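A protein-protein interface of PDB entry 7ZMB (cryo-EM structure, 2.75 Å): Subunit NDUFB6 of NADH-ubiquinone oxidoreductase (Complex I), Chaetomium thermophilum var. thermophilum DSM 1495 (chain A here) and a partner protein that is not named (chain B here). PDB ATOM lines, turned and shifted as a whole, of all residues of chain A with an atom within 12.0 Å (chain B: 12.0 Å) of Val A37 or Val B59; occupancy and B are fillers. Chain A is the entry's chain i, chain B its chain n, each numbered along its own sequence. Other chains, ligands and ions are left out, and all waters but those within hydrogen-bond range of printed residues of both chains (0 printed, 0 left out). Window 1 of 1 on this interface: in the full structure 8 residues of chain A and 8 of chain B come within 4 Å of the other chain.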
ATOM      1  N   LYS A  28       1.802   9.950 -16.217  1.00  0.00           N
ATOM      2  CA  LYS A  28       0.443   9.468 -16.432  1.00  0.00           C
ATOM      3  C   LYS A  28       0.368   7.944 -16.378  1.00  0.00           C
ATOM      4  O   LYS A  28      -0.427   7.385 -15.618  1.00  0.00           O
ATOM      5  CB  LYS A  28      -0.093   9.986 -17.771  1.00  0.00           C
ATOM      6  CG  LYS A  28      -0.607  11.412 -17.725  1.00  0.00           C
ATOM      7  CD  LYS A  28      -1.431  11.732 -18.961  1.00  0.00           C
ATOM      8  CE  LYS A  28      -1.853  13.190 -18.985  1.00  0.00           C
ATOM      9  NZ  LYS A  28      -0.692  14.097 -19.194  1.00  0.00           N
ATOM     10  N   GLN A  29       1.177   7.263 -17.189  1.00  0.00           N
ATOM     11  CA  GLN A  29       1.179   5.806 -17.159  1.00  0.00           C
ATOM     12  C   GLN A  29       1.645   5.293 -15.804  1.00  0.00           C
ATOM     13  O   GLN A  29       1.112   4.303 -15.290  1.00  0.00           O
ATOM     14  CB  GLN A  29       2.051   5.250 -18.289  1.00  0.00           C
ATOM     15  CG  GLN A  29       3.531   5.578 -18.186  1.00  0.00           C
ATOM     16  CD  GLN A  29       4.326   5.051 -19.363  1.00  0.00           C
ATOM     17  OE1 GLN A  29       3.785   4.388 -20.246  1.00  0.00           O
ATOM     18  NE2 GLN A  29       5.621   5.342 -19.379  1.00  0.00           N
ATOM     19  N   ASN A  30       2.631   5.961 -15.204  1.00  0.00           N
ATOM     20  CA  ASN A  30       3.030   5.620 -13.845  1.00  0.00           C
ATOM     21  C   ASN A  30       1.890   5.858 -12.866  1.00  0.00           C
ATOM     22  O   ASN A  30       1.665   5.053 -11.957  1.00  0.00           O
ATOM     23  CB  ASN A  30       4.266   6.422 -13.446  1.00  0.00           C
ATOM     24  CG  ASN A  30       5.539   5.856 -14.033  1.00  0.00           C
ATOM     25  OD1 ASN A  30       6.289   6.554 -14.714  1.00  0.00           O
ATOM     26  ND2 ASN A  30       5.788   4.577 -13.776  1.00  0.00           N
ATOM     27  N   THR A  31       1.155   6.960 -13.038  1.00  0.00           N
ATOM     28  CA  THR A  31      -0.036   7.173 -12.224  1.00  0.00           C
ATOM     29  C   THR A  31      -1.051   6.069 -12.464  1.00  0.00           C
ATOM     30  O   THR A  31      -1.655   5.550 -11.518  1.00  0.00           O
ATOM     31  CB  THR A  31      -0.655   8.539 -12.523  1.00  0.00           C
ATOM     32  OG1 THR A  31       0.261   9.578 -12.158  1.00  0.00           O
ATOM     33  CG2 THR A  31      -1.951   8.719 -11.746  1.00  0.00           C
ATOM     34  N   ALA A  32      -1.246   5.690 -13.728  1.00  0.00           N
ATOM     35  CA  ALA A  32      -2.134   4.575 -14.033  1.00  0.00           C
ATOM     36  C   ALA A  32      -1.615   3.280 -13.424  1.00  0.00           C
ATOM     37  O   ALA A  32      -2.395   2.478 -12.899  1.00  0.00           O
ATOM     38  CB  ALA A  32      -2.298   4.434 -15.545  1.00  0.00           C
ATOM     39  N   ILE A  33      -0.302   3.061 -13.481  1.00  0.00           N
ATOM     40  CA  ILE A  33       0.274   1.839 -12.923  1.00  0.00           C
ATOM     41  C   ILE A  33       0.021   1.772 -11.425  1.00  0.00           C
ATOM     42  O   ILE A  33      -0.391   0.737 -10.893  1.00  0.00           O
ATOM     43  CB  ILE A  33       1.775   1.753 -13.251  1.00  0.00           C
ATOM     44  CG1 ILE A  33       1.975   1.277 -14.690  1.00  0.00           C
ATOM     45  CG2 ILE A  33       2.482   0.824 -12.282  1.00  0.00           C
ATOM     46  CD1 ILE A  33       3.422   1.046 -15.062  1.00  0.00           C
ATOM     47  N   PHE A  34       0.257   2.878 -10.721  1.00  0.00           N
ATOM     48  CA  PHE A  34      -0.022   2.907  -9.289  1.00  0.00           C
ATOM     49  C   PHE A  34      -1.515   2.846  -9.004  1.00  0.00           C
ATOM     50  O   PHE A  34      -1.931   2.213  -8.028  1.00  0.00           O
ATOM     51  CB  PHE A  34       0.588   4.158  -8.660  1.00  0.00           C
ATOM     52  CG  PHE A  34       2.041   4.021  -8.336  1.00  0.00           C
ATOM     53  CD1 PHE A  34       3.004   4.313  -9.284  1.00  0.00           C
ATOM     54  CD2 PHE A  34       2.446   3.591  -7.090  1.00  0.00           C
ATOM     55  CE1 PHE A  34       4.344   4.181  -8.991  1.00  0.00           C
ATOM     56  CE2 PHE A  34       3.778   3.458  -6.790  1.00  0.00           C
ATOM     57  CZ  PHE A  34       4.730   3.750  -7.740  1.00  0.00           C
ATOM     58  N   GLY A  35      -2.333   3.490  -9.840  1.00  0.00           N
ATOM     59  CA  GLY A  35      -3.769   3.486  -9.620  1.00  0.00           C
ATOM     60  C   GLY A  35      -4.380   2.103  -9.673  1.00  0.00           C
ATOM     61  O   GLY A  35      -5.351   1.822  -8.967  1.00  0.00           O
ATOM     62  N   LEU A  36      -3.838   1.226 -10.518  1.00  0.00           N
ATOM     63  CA  LEU A  36      -4.292  -0.160 -10.527  1.00  0.00           C
ATOM     64  C   LEU A  36      -3.987  -0.842  -9.200  1.00  0.00           C
ATOM     65  O   LEU A  36      -4.784  -1.651  -8.712  1.00  0.00           O
ATOM     66  CB  LEU A  36      -3.650  -0.920 -11.686  1.00  0.00           C
ATOM     67  CG  LEU A  36      -4.421  -0.984 -13.009  1.00  0.00           C
ATOM     68  CD1 LEU A  36      -5.691  -1.802 -12.841  1.00  0.00           C
ATOM     69  CD2 LEU A  36      -4.749   0.404 -13.536  1.00  0.00           C
ATOM     70  N   VAL A  37      -2.838  -0.526  -8.602  1.00  0.00           N
ATOM     71  CA  VAL A  37      -2.463  -1.144  -7.335  1.00  0.00           C
ATOM     72  C   VAL A  37      -3.449  -0.765  -6.241  1.00  0.00           C
ATOM     73  O   VAL A  37      -3.860  -1.609  -5.437  1.00  0.00           O
ATOM     74  CB  VAL A  37      -1.024  -0.760  -6.951  1.00  0.00           C
ATOM     75  CG1 VAL A  37      -0.533  -1.641  -5.818  1.00  0.00           C
ATOM     76  CG2 VAL A  37      -0.108  -0.880  -8.154  1.00  0.00           C
ATOM     77  N   ILE A  38      -3.834   0.513  -6.180  1.00  0.00           N
ATOM     78  CA  ILE A  38      -4.765   0.950  -5.145  1.00  0.00           C
ATOM     79  C   ILE A  38      -6.106   0.259  -5.318  1.00  0.00           C
ATOM     80  O   ILE A  38      -6.685  -0.255  -4.357  1.00  0.00           O
ATOM     81  CB  ILE A  38      -4.913   2.479  -5.156  1.00  0.00           C
ATOM     82  CG1 ILE A  38      -3.585   3.142  -4.826  1.00  0.00           C
ATOM     83  CG2 ILE A  38      -5.960   2.909  -4.157  1.00  0.00           C
ATOM     84  CD1 ILE A  38      -3.592   4.616  -5.065  1.00  0.00           C
ATOM     85  N   PHE A  39      -6.607   0.215  -6.550  1.00  0.00           N
ATOM     86  CA  PHE A  39      -7.837  -0.520  -6.821  1.00  0.00           C
ATOM     87  C   PHE A  39      -7.671  -2.000  -6.510  1.00  0.00           C
ATOM     88  O   PHE A  39      -8.558  -2.619  -5.913  1.00  0.00           O
ATOM     89  CB  PHE A  39      -8.250  -0.317  -8.281  1.00  0.00           C
ATOM     90  CG  PHE A  39      -9.569  -0.945  -8.641  1.00  0.00           C
ATOM     91  CD1 PHE A  39      -9.661  -2.297  -8.930  1.00  0.00           C
ATOM     92  CD2 PHE A  39     -10.713  -0.169  -8.730  1.00  0.00           C
ATOM     93  CE1 PHE A  39     -10.872  -2.867  -9.273  1.00  0.00           C
ATOM     94  CE2 PHE A  39     -11.927  -0.735  -9.072  1.00  0.00           C
ATOM     95  CZ  PHE A  39     -12.006  -2.085  -9.345  1.00  0.00           C
ATOM     96  N   GLY A  40      -6.538  -2.582  -6.906  1.00  0.00           N
ATOM     97  CA  GLY A  40      -6.360  -4.015  -6.749  1.00  0.00           C
ATOM     98  C   GLY A  40      -6.480  -4.463  -5.306  1.00  0.00           C
ATOM     99  O   GLY A  40      -7.172  -5.438  -5.000  1.00  0.00           O
ATOM    100  N   ILE A  41      -5.824  -3.746  -4.396  1.00  0.00           N
ATOM    101  CA  ILE A  41      -5.886  -4.140  -2.996  1.00  0.00           C
ATOM    102  C   ILE A  41      -7.076  -3.527  -2.274  1.00  0.00           C
ATOM    103  O   ILE A  41      -7.401  -3.958  -1.165  1.00  0.00           O
ATOM    104  CB  ILE A  41      -4.565  -3.804  -2.286  1.00  0.00           C
ATOM    105  CG1 ILE A  41      -4.433  -2.308  -2.043  1.00  0.00           C
ATOM    106  CG2 ILE A  41      -3.386  -4.305  -3.099  1.00  0.00           C
ATOM    107  CD1 ILE A  41      -3.146  -1.957  -1.357  1.00  0.00           C
ATOM    108  N   THR A  42      -7.746  -2.541  -2.866  1.00  0.00           N
ATOM    109  CA  THR A  42      -8.967  -2.023  -2.263  1.00  0.00           C
ATOM    110  C   THR A  42     -10.075  -3.065  -2.287  1.00  0.00           C
ATOM    111  O   THR A  42     -10.696  -3.352  -1.256  1.00  0.00           O
ATOM    112  CB  THR A  42      -9.416  -0.756  -2.988  1.00  0.00           C
ATOM    113  OG1 THR A  42      -8.462   0.289  -2.764  1.00  0.00           O
ATOM    114  CG2 THR A  42     -10.794  -0.323  -2.512  1.00  0.00           C
ATOM    115  N   ALA A  43     -10.343  -3.643  -3.459  1.00  0.00           N
ATOM    116  CA  ALA A  43     -11.301  -4.738  -3.529  1.00  0.00           C
ATOM    117  C   ALA A  43     -10.794  -5.934  -2.743  1.00  0.00           C
ATOM    118  O   ALA A  43     -11.583  -6.702  -2.180  1.00  0.00           O
ATOM    119  CB  ALA A  43     -11.567  -5.117  -4.986  1.00  0.00           C
ATOM    120  N   MET A  44      -9.472  -6.103  -2.698  1.00  0.00           N
ATOM    121  CA  MET A  44      -8.874  -7.110  -1.835  1.00  0.00           C
ATOM    122  C   MET A  44      -9.247  -6.854  -0.385  1.00  0.00           C
ATOM    123  O   MET A  44      -9.612  -7.779   0.349  1.00  0.00           O
ATOM    124  CB  MET A  44      -7.363  -7.085  -2.020  1.00  0.00           C
ATOM    125  CG  MET A  44      -6.607  -8.290  -1.547  1.00  0.00           C
ATOM    126  SD  MET A  44      -5.206  -8.469  -2.660  1.00  0.00           S
ATOM    127  CE  MET A  44      -4.687 -10.121  -2.278  1.00  0.00           C
ATOM    128  N   VAL A  45      -9.162  -5.598   0.045  1.00  0.00           N
ATOM    129  CA  VAL A  45      -9.724  -5.208   1.334  1.00  0.00           C
ATOM    130  C   VAL A  45     -11.237  -5.395   1.338  1.00  0.00           C
ATOM    131  O   VAL A  45     -11.809  -5.937   2.291  1.00  0.00           O
ATOM    132  CB  VAL A  45      -9.338  -3.759   1.664  1.00  0.00           C
ATOM    133  CG1 VAL A  45     -10.076  -3.311   2.894  1.00  0.00           C
ATOM    134  CG2 VAL A  45      -7.847  -3.659   1.890  1.00  0.00           C
ATOM    135  N   TRP A  46     -11.906  -4.947   0.273  1.00  0.00           N
ATOM    136  CA  TRP A  46     -13.360  -5.043   0.227  1.00  0.00           C
ATOM    137  C   TRP A  46     -13.813  -6.491   0.323  1.00  0.00           C
ATOM    138  O   TRP A  46     -14.822  -6.789   0.969  1.00  0.00           O
ATOM    139  CB  TRP A  46     -13.897  -4.393  -1.051  1.00  0.00           C
ATOM    140  CG  TRP A  46     -15.360  -4.040  -1.004  1.00  0.00           C
ATOM    141  CD1 TRP A  46     -16.382  -4.829  -0.570  1.00  0.00           C
ATOM    142  CD2 TRP A  46     -15.958  -2.812  -1.433  1.00  0.00           C
ATOM    143  NE1 TRP A  46     -17.578  -4.167  -0.690  1.00  0.00           N
ATOM    144  CE2 TRP A  46     -17.344  -2.927  -1.219  1.00  0.00           C
ATOM    145  CE3 TRP A  46     -15.456  -1.625  -1.972  1.00  0.00           C
ATOM    146  CZ2 TRP A  46     -18.232  -1.904  -1.524  1.00  0.00           C
ATOM    147  CZ3 TRP A  46     -16.339  -0.611  -2.274  1.00  0.00           C
ATOM    148  CH2 TRP A  46     -17.711  -0.755  -2.048  1.00  0.00           C
ATOM    149  N   PRO B  50      11.790   5.658 -13.875  1.00  0.00           N
ATOM    150  CA  PRO B  50      11.447   4.235 -13.884  1.00  0.00           C
ATOM    151  C   PRO B  50      10.555   3.843 -12.700  1.00  0.00           C
ATOM    152  O   PRO B  50      10.621   4.475 -11.670  1.00  0.00           O
ATOM    153  CB  PRO B  50      12.804   3.544 -13.711  1.00  0.00           C
ATOM    154  CG  PRO B  50      13.662   4.571 -13.010  1.00  0.00           C
ATOM    155  CD  PRO B  50      13.199   5.900 -13.565  1.00  0.00           C
ATOM    156  N   LEU B  51       9.731   2.818 -12.890  1.00  0.00           N
ATOM    157  CA  LEU B  51       8.905   2.321 -11.766  1.00  0.00           C
ATOM    158  C   LEU B  51       9.815   2.084 -10.569  1.00  0.00           C
ATOM    159  O   LEU B  51       9.391   2.444  -9.446  1.00  0.00           O
ATOM    160  CB  LEU B  51       8.159   1.051 -12.154  1.00  0.00           C
ATOM    161  CG  LEU B  51       6.740   1.285 -12.658  1.00  0.00           C
ATOM    162  CD1 LEU B  51       6.086  -0.032 -13.041  1.00  0.00           C
ATOM    163  CD2 LEU B  51       5.917   2.010 -11.606  1.00  0.00           C
ATOM    164  N   GLY B  52      11.009   1.544 -10.787  1.00  0.00           N
ATOM    165  CA  GLY B  52      11.940   1.404  -9.659  1.00  0.00           C
ATOM    166  C   GLY B  52      11.773   0.090  -8.926  1.00  0.00           C
ATOM    167  O   GLY B  52      10.625  -0.379  -8.795  1.00  0.00           O
ATOM    168  N   ALA B  53      12.877  -0.477  -8.439  1.00  0.00           N
ATOM    169  CA  ALA B  53      12.854  -1.769  -7.764  1.00  0.00           C
ATOM    170  C   ALA B  53      12.003  -1.730  -6.502  1.00  0.00           C
ATOM    171  O   ALA B  53      11.422  -2.751  -6.118  1.00  0.00           O
ATOM    172  CB  ALA B  53      14.277  -2.214  -7.433  1.00  0.00           C
ATOM    173  N   ALA B  54      11.920  -0.570  -5.847  1.00  0.00           N
ATOM    174  CA  ALA B  54      11.133  -0.465  -4.621  1.00  0.00           C
ATOM    175  C   ALA B  54       9.660  -0.732  -4.886  1.00  0.00           C
ATOM    176  O   ALA B  54       8.980  -1.366  -4.070  1.00  0.00           O
ATOM    177  CB  ALA B  54      11.320   0.915  -3.994  1.00  0.00           C
ATOM    178  N   PHE B  55       9.147  -0.250  -6.019  1.00  0.00           N
ATOM    179  CA  PHE B  55       7.745  -0.478  -6.352  1.00  0.00           C
ATOM    180  C   PHE B  55       7.448  -1.965  -6.484  1.00  0.00           C
ATOM    181  O   PHE B  55       6.404  -2.441  -6.023  1.00  0.00           O
ATOM    182  CB  PHE B  55       7.392   0.259  -7.643  1.00  0.00           C
ATOM    183  CG  PHE B  55       6.131  -0.225  -8.291  1.00  0.00           C
ATOM    184  CD1 PHE B  55       4.895   0.143  -7.792  1.00  0.00           C
ATOM    185  CD2 PHE B  55       6.180  -1.043  -9.405  1.00  0.00           C
ATOM    186  CE1 PHE B  55       3.732  -0.300  -8.388  1.00  0.00           C
ATOM    187  CE2 PHE B  55       5.022  -1.489 -10.004  1.00  0.00           C
ATOM    188  CZ  PHE B  55       3.796  -1.118  -9.496  1.00  0.00           C
ATOM    189  N   TYR B  56       8.357  -2.716  -7.106  1.00  0.00           N
ATOM    190  CA  TYR B  56       8.128  -4.144  -7.297  1.00  0.00           C
ATOM    191  C   TYR B  56       8.261  -4.908  -5.986  1.00  0.00           C
ATOM    192  O   TYR B  56       7.549  -5.894  -5.763  1.00  0.00           O
ATOM    193  CB  TYR B  56       9.097  -4.687  -8.344  1.00  0.00           C
ATOM    194  CG  TYR B  56       8.874  -4.098  -9.716  1.00  0.00           C
ATOM    195  CD1 TYR B  56       7.627  -4.157 -10.321  1.00  0.00           C
ATOM    196  CD2 TYR B  56       9.904  -3.471 -10.399  1.00  0.00           C
ATOM    197  CE1 TYR B  56       7.414  -3.617 -11.571  1.00  0.00           C
ATOM    198  CE2 TYR B  56       9.701  -2.927 -11.651  1.00  0.00           C
ATOM    199  CZ  TYR B  56       8.454  -3.002 -12.231  1.00  0.00           C
ATOM    200  OH  TYR B  56       8.245  -2.462 -13.479  1.00  0.00           O
ATOM    201  N   ILE B  57       9.169  -4.477  -5.109  1.00  0.00           N
ATOM    202  CA  ILE B  57       9.346  -5.158  -3.830  1.00  0.00           C
ATOM    203  C   ILE B  57       8.092  -5.023  -2.976  1.00  0.00           C
ATOM    204  O   ILE B  57       7.598  -6.001  -2.404  1.00  0.00           O
ATOM    205  CB  ILE B  57      10.585  -4.613  -3.098  1.00  0.00           C
ATOM    206  CG1 ILE B  57      11.860  -4.999  -3.847  1.00  0.00           C
ATOM    207  CG2 ILE B  57      10.632  -5.130  -1.673  1.00  0.00           C
ATOM    208  CD1 ILE B  57      13.116  -4.414  -3.249  1.00  0.00           C
ATOM    209  N   ALA B  58       7.557  -3.804  -2.880  1.00  0.00           N
ATOM    210  CA  ALA B  58       6.358  -3.584  -2.079  1.00  0.00           C
ATOM    211  C   ALA B  58       5.157  -4.309  -2.673  1.00  0.00           C
ATOM    212  O   ALA B  58       4.428  -5.009  -1.962  1.00  0.00           O
ATOM    213  CB  ALA B  58       6.078  -2.087  -1.956  1.00  0.00           C
ATOM    214  N   VAL B  59       4.936  -4.149  -3.979  1.00  0.00           N
ATOM    215  CA  VAL B  59       3.829  -4.843  -4.633  1.00  0.00           C
ATOM    216  C   VAL B  59       4.049  -6.347  -4.594  1.00  0.00           C
ATOM    217  O   VAL B  59       3.129  -7.119  -4.297  1.00  0.00           O
ATOM    218  CB  VAL B  59       3.652  -4.328  -6.072  1.00  0.00           C
ATOM    219  CG1 VAL B  59       2.671  -5.205  -6.833  1.00  0.00           C
ATOM    220  CG2 VAL B  59       3.178  -2.888  -6.057  1.00  0.00           C
ATOM    221  N   GLY B  60       5.272  -6.788  -4.892  1.00  0.00           N
ATOM    222  CA  GLY B  60       5.571  -8.208  -4.815  1.00  0.00           C
ATOM    223  C   GLY B  60       5.398  -8.765  -3.416  1.00  0.00           C
ATOM    224  O   GLY B  60       4.874  -9.866  -3.237  1.00  0.00           O
ATOM    225  N   GLY B  61       5.834  -8.010  -2.406  1.00  0.00           N
ATOM    226  CA  GLY B  61       5.646  -8.452  -1.034  1.00  0.00           C
ATOM    227  C   GLY B  61       4.182  -8.559  -0.651  1.00  0.00           C
ATOM    228  O   GLY B  61       3.767  -9.527  -0.009  1.00  0.00           O
ATOM    229  N   ILE B  62       3.381  -7.564  -1.037  1.00  0.00           N
ATOM    230  CA  ILE B  62       1.946  -7.622  -0.774  1.00  0.00           C
ATOM    231  C   ILE B  62       1.311  -8.768  -1.550  1.00  0.00           C
ATOM    232  O   ILE B  62       0.497  -9.528  -1.010  1.00  0.00           O
ATOM    233  CB  ILE B  62       1.286  -6.274  -1.112  1.00  0.00           C
ATOM    234  CG1 ILE B  62       1.747  -5.194  -0.132  1.00  0.00           C
ATOM    235  CG2 ILE B  62      -0.229  -6.400  -1.087  1.00  0.00           C
ATOM    236  CD1 ILE B  62       1.371  -3.793  -0.554  1.00  0.00           C
ATOM    237  N   ALA B  63       1.669  -8.910  -2.828  1.00  0.00           N
ATOM    238  CA  ALA B  63       1.120  -9.995  -3.635  1.00  0.00           C
ATOM    239  C   ALA B  63       1.537 -11.354  -3.091  1.00  0.00           C
ATOM    240  O   ALA B  63       0.723 -12.282  -3.024  1.00  0.00           O
ATOM    241  CB  ALA B  63       1.556  -9.843  -5.091  1.00  0.00           C
ATOM    242  N   SER B  64       2.805 -11.492  -2.697  1.00  0.00           N
ATOM    243  CA  SER B  64       3.276 -12.759  -2.145  1.00  0.00           C
ATOM    244  C   SER B  64       2.562 -13.085  -0.840  1.00  0.00           C
ATOM    245  O   SER B  64       2.241 -14.248  -0.571  1.00  0.00           O
ATOM    246  CB  SER B  64       4.789 -12.714  -1.936  1.00  0.00           C
ATOM    247  OG  SER B  64       5.470 -12.644  -3.175  1.00  0.00           O
ATOM    248  N   SER B  65       2.300 -12.063  -0.019  1.00  0.00           N
ATOM    249  CA  SER B  65       1.685 -12.294   1.285  1.00  0.00           C
ATOM    250  C   SER B  65       0.352 -13.018   1.151  1.00  0.00           C
ATOM    251  O   SER B  65       0.062 -13.945   1.915  1.00  0.00           O
ATOM    252  CB  SER B  65       1.500 -10.963   2.014  1.00  0.00           C
ATOM    253  OG  SER B  65       2.735 -10.287   2.171  1.00  0.00           O
ATOM    254  N   PHE B  66      -0.469 -12.612   0.182  1.00  0.00           N
ATOM    255  CA  PHE B  66      -1.738 -13.295  -0.044  1.00  0.00           C
ATOM    256  C   PHE B  66      -1.520 -14.730  -0.503  1.00  0.00           C
ATOM    257  O   PHE B  66      -2.227 -15.646  -0.064  1.00  0.00           O
ATOM    258  CB  PHE B  66      -2.560 -12.525  -1.072  1.00  0.00           C
ATOM    259  CG  PHE B  66      -3.892 -13.146  -1.382  1.00  0.00           C
ATOM    260  CD1 PHE B  66      -4.911 -13.131  -0.445  1.00  0.00           C
ATOM    261  CD2 PHE B  66      -4.140 -13.709  -2.623  1.00  0.00           C
ATOM    262  CE1 PHE B  66      -6.142 -13.687  -0.728  1.00  0.00           C
ATOM    263  CE2 PHE B  66      -5.371 -14.267  -2.913  1.00  0.00           C
ATOM    264  CZ  PHE B  66      -6.372 -14.256  -1.964  1.00  0.00           C
ATOM    265  N   VAL B  67      -0.547 -14.945  -1.388  1.00  0.00           N
ATOM    266  CA  VAL B  67      -0.282 -16.288  -1.899  1.00  0.00           C
ATOM    267  C   VAL B  67       0.184 -17.201  -0.773  1.00  0.00           C
ATOM    268  O   VAL B  67      -0.264 -18.347  -0.650  1.00  0.00           O
ATOM    269  CB  VAL B  67       0.746 -16.231  -3.043  1.00  0.00           C
ATOM    270  CG1 VAL B  67       1.198 -17.630  -3.419  1.00  0.00           C
ATOM    271  CG2 VAL B  67       0.161 -15.507  -4.246  1.00  0.00           C
ATOM    272  N   ILE B  68       1.093 -16.704   0.067  1.00  0.00           N
ATOM    273  CA  ILE B  68       1.606 -17.508   1.171  1.00  0.00           C
ATOM    274  C   ILE B  68       0.511 -17.767   2.198  1.00  0.00           C
ATOM    275  O   ILE B  68       0.445 -18.845   2.800  1.00  0.00           O
ATOM    276  CB  ILE B  68       2.827 -16.819   1.803  1.00  0.00           C
ATOM    277  CG1 ILE B  68       3.880 -16.537   0.733  1.00  0.00           C
ATOM    278  CG2 ILE B  68       3.417 -17.687   2.900  1.00  0.00           C
ATOM    279  CD1 ILE B  68       4.856 -15.451   1.113  1.00  0.00           C
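ND2 of Asn A30 touches CD2 of Leu B51, at 3.4 Å. Leu B51 touches Ile A33 (CD1 to CD1, 3.5 Å). Ile A33 touches Phe B55. Leu B51 touches Phe A34. Phe A34 touches Phe B55 (CZ to CD1, 3.6 Å). Phe B55 touches Val A37 (CE1 to CG2, 3.9 Å). Val B59 touches Val A37. Phe B66 touches Met A44 (CG to CE, 3.3 Å).
Printed residues of chain B within 4 Å of Asn A30: Leu B51 (3.4 Å). Printed residues of chain B within 4 Å of Ile A33: Leu B51 and Phe B55. Phe A34 touches just these residues of chain B: Leu B51 and Phe B55. No residue of chain B comes within 4 Å of Gly A35. No residue of chain B comes within 4 Å of Leu A36. No residue of chain B comes within 4 Å of Ile A38. Gly A40 touches none of the printed residues of chain B. Ile A41 touches none of the printed residues of chain B. Thr A42 touches none of the printed residues of chain B. Phe B55 touches just these residues of chain A: Ile A33, Phe A34 and Val A37. No residue of chain A comes within 4 Å of Ala B58. Val B59 touches just one residue of chain A: Val A37 (3.9 Å). No residue of chain A comes within 4 Å of Gly B60. No residue of chain A comes within 4 Å of Gly B61. No residue of chain A comes within 4 Å of Ile B62. No residue of chain A comes within 4 Å of Ala B63. Of the printed residues of chain A, Phe B66 touches Met A44 (3.3 Å). The nearest residue of chain A that does not touch Val B59 is Phe A34 (6.4 Å). The nearest printed residue of chain A that does not touch Phe B66 is Ile A41 (8.5 Å).
Of the 19 printed residues of chain A, 5 touch a printed residue of chain B. Printed residues of chain A that touch a printed residue of chain B: Asn A30, Ile A33, Phe A34, Val A37 and Met A44. Hydrophobic or aromatic side chains of chain B within 4 Å of the printed part of chain A: Leu B51, Phe B55, Val B59 and Phe B66. Along chain B the printed residues that touch a printed residue of chain A span positions 51 to 66. Among the printed residues, 8 pairs touch across the chains.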
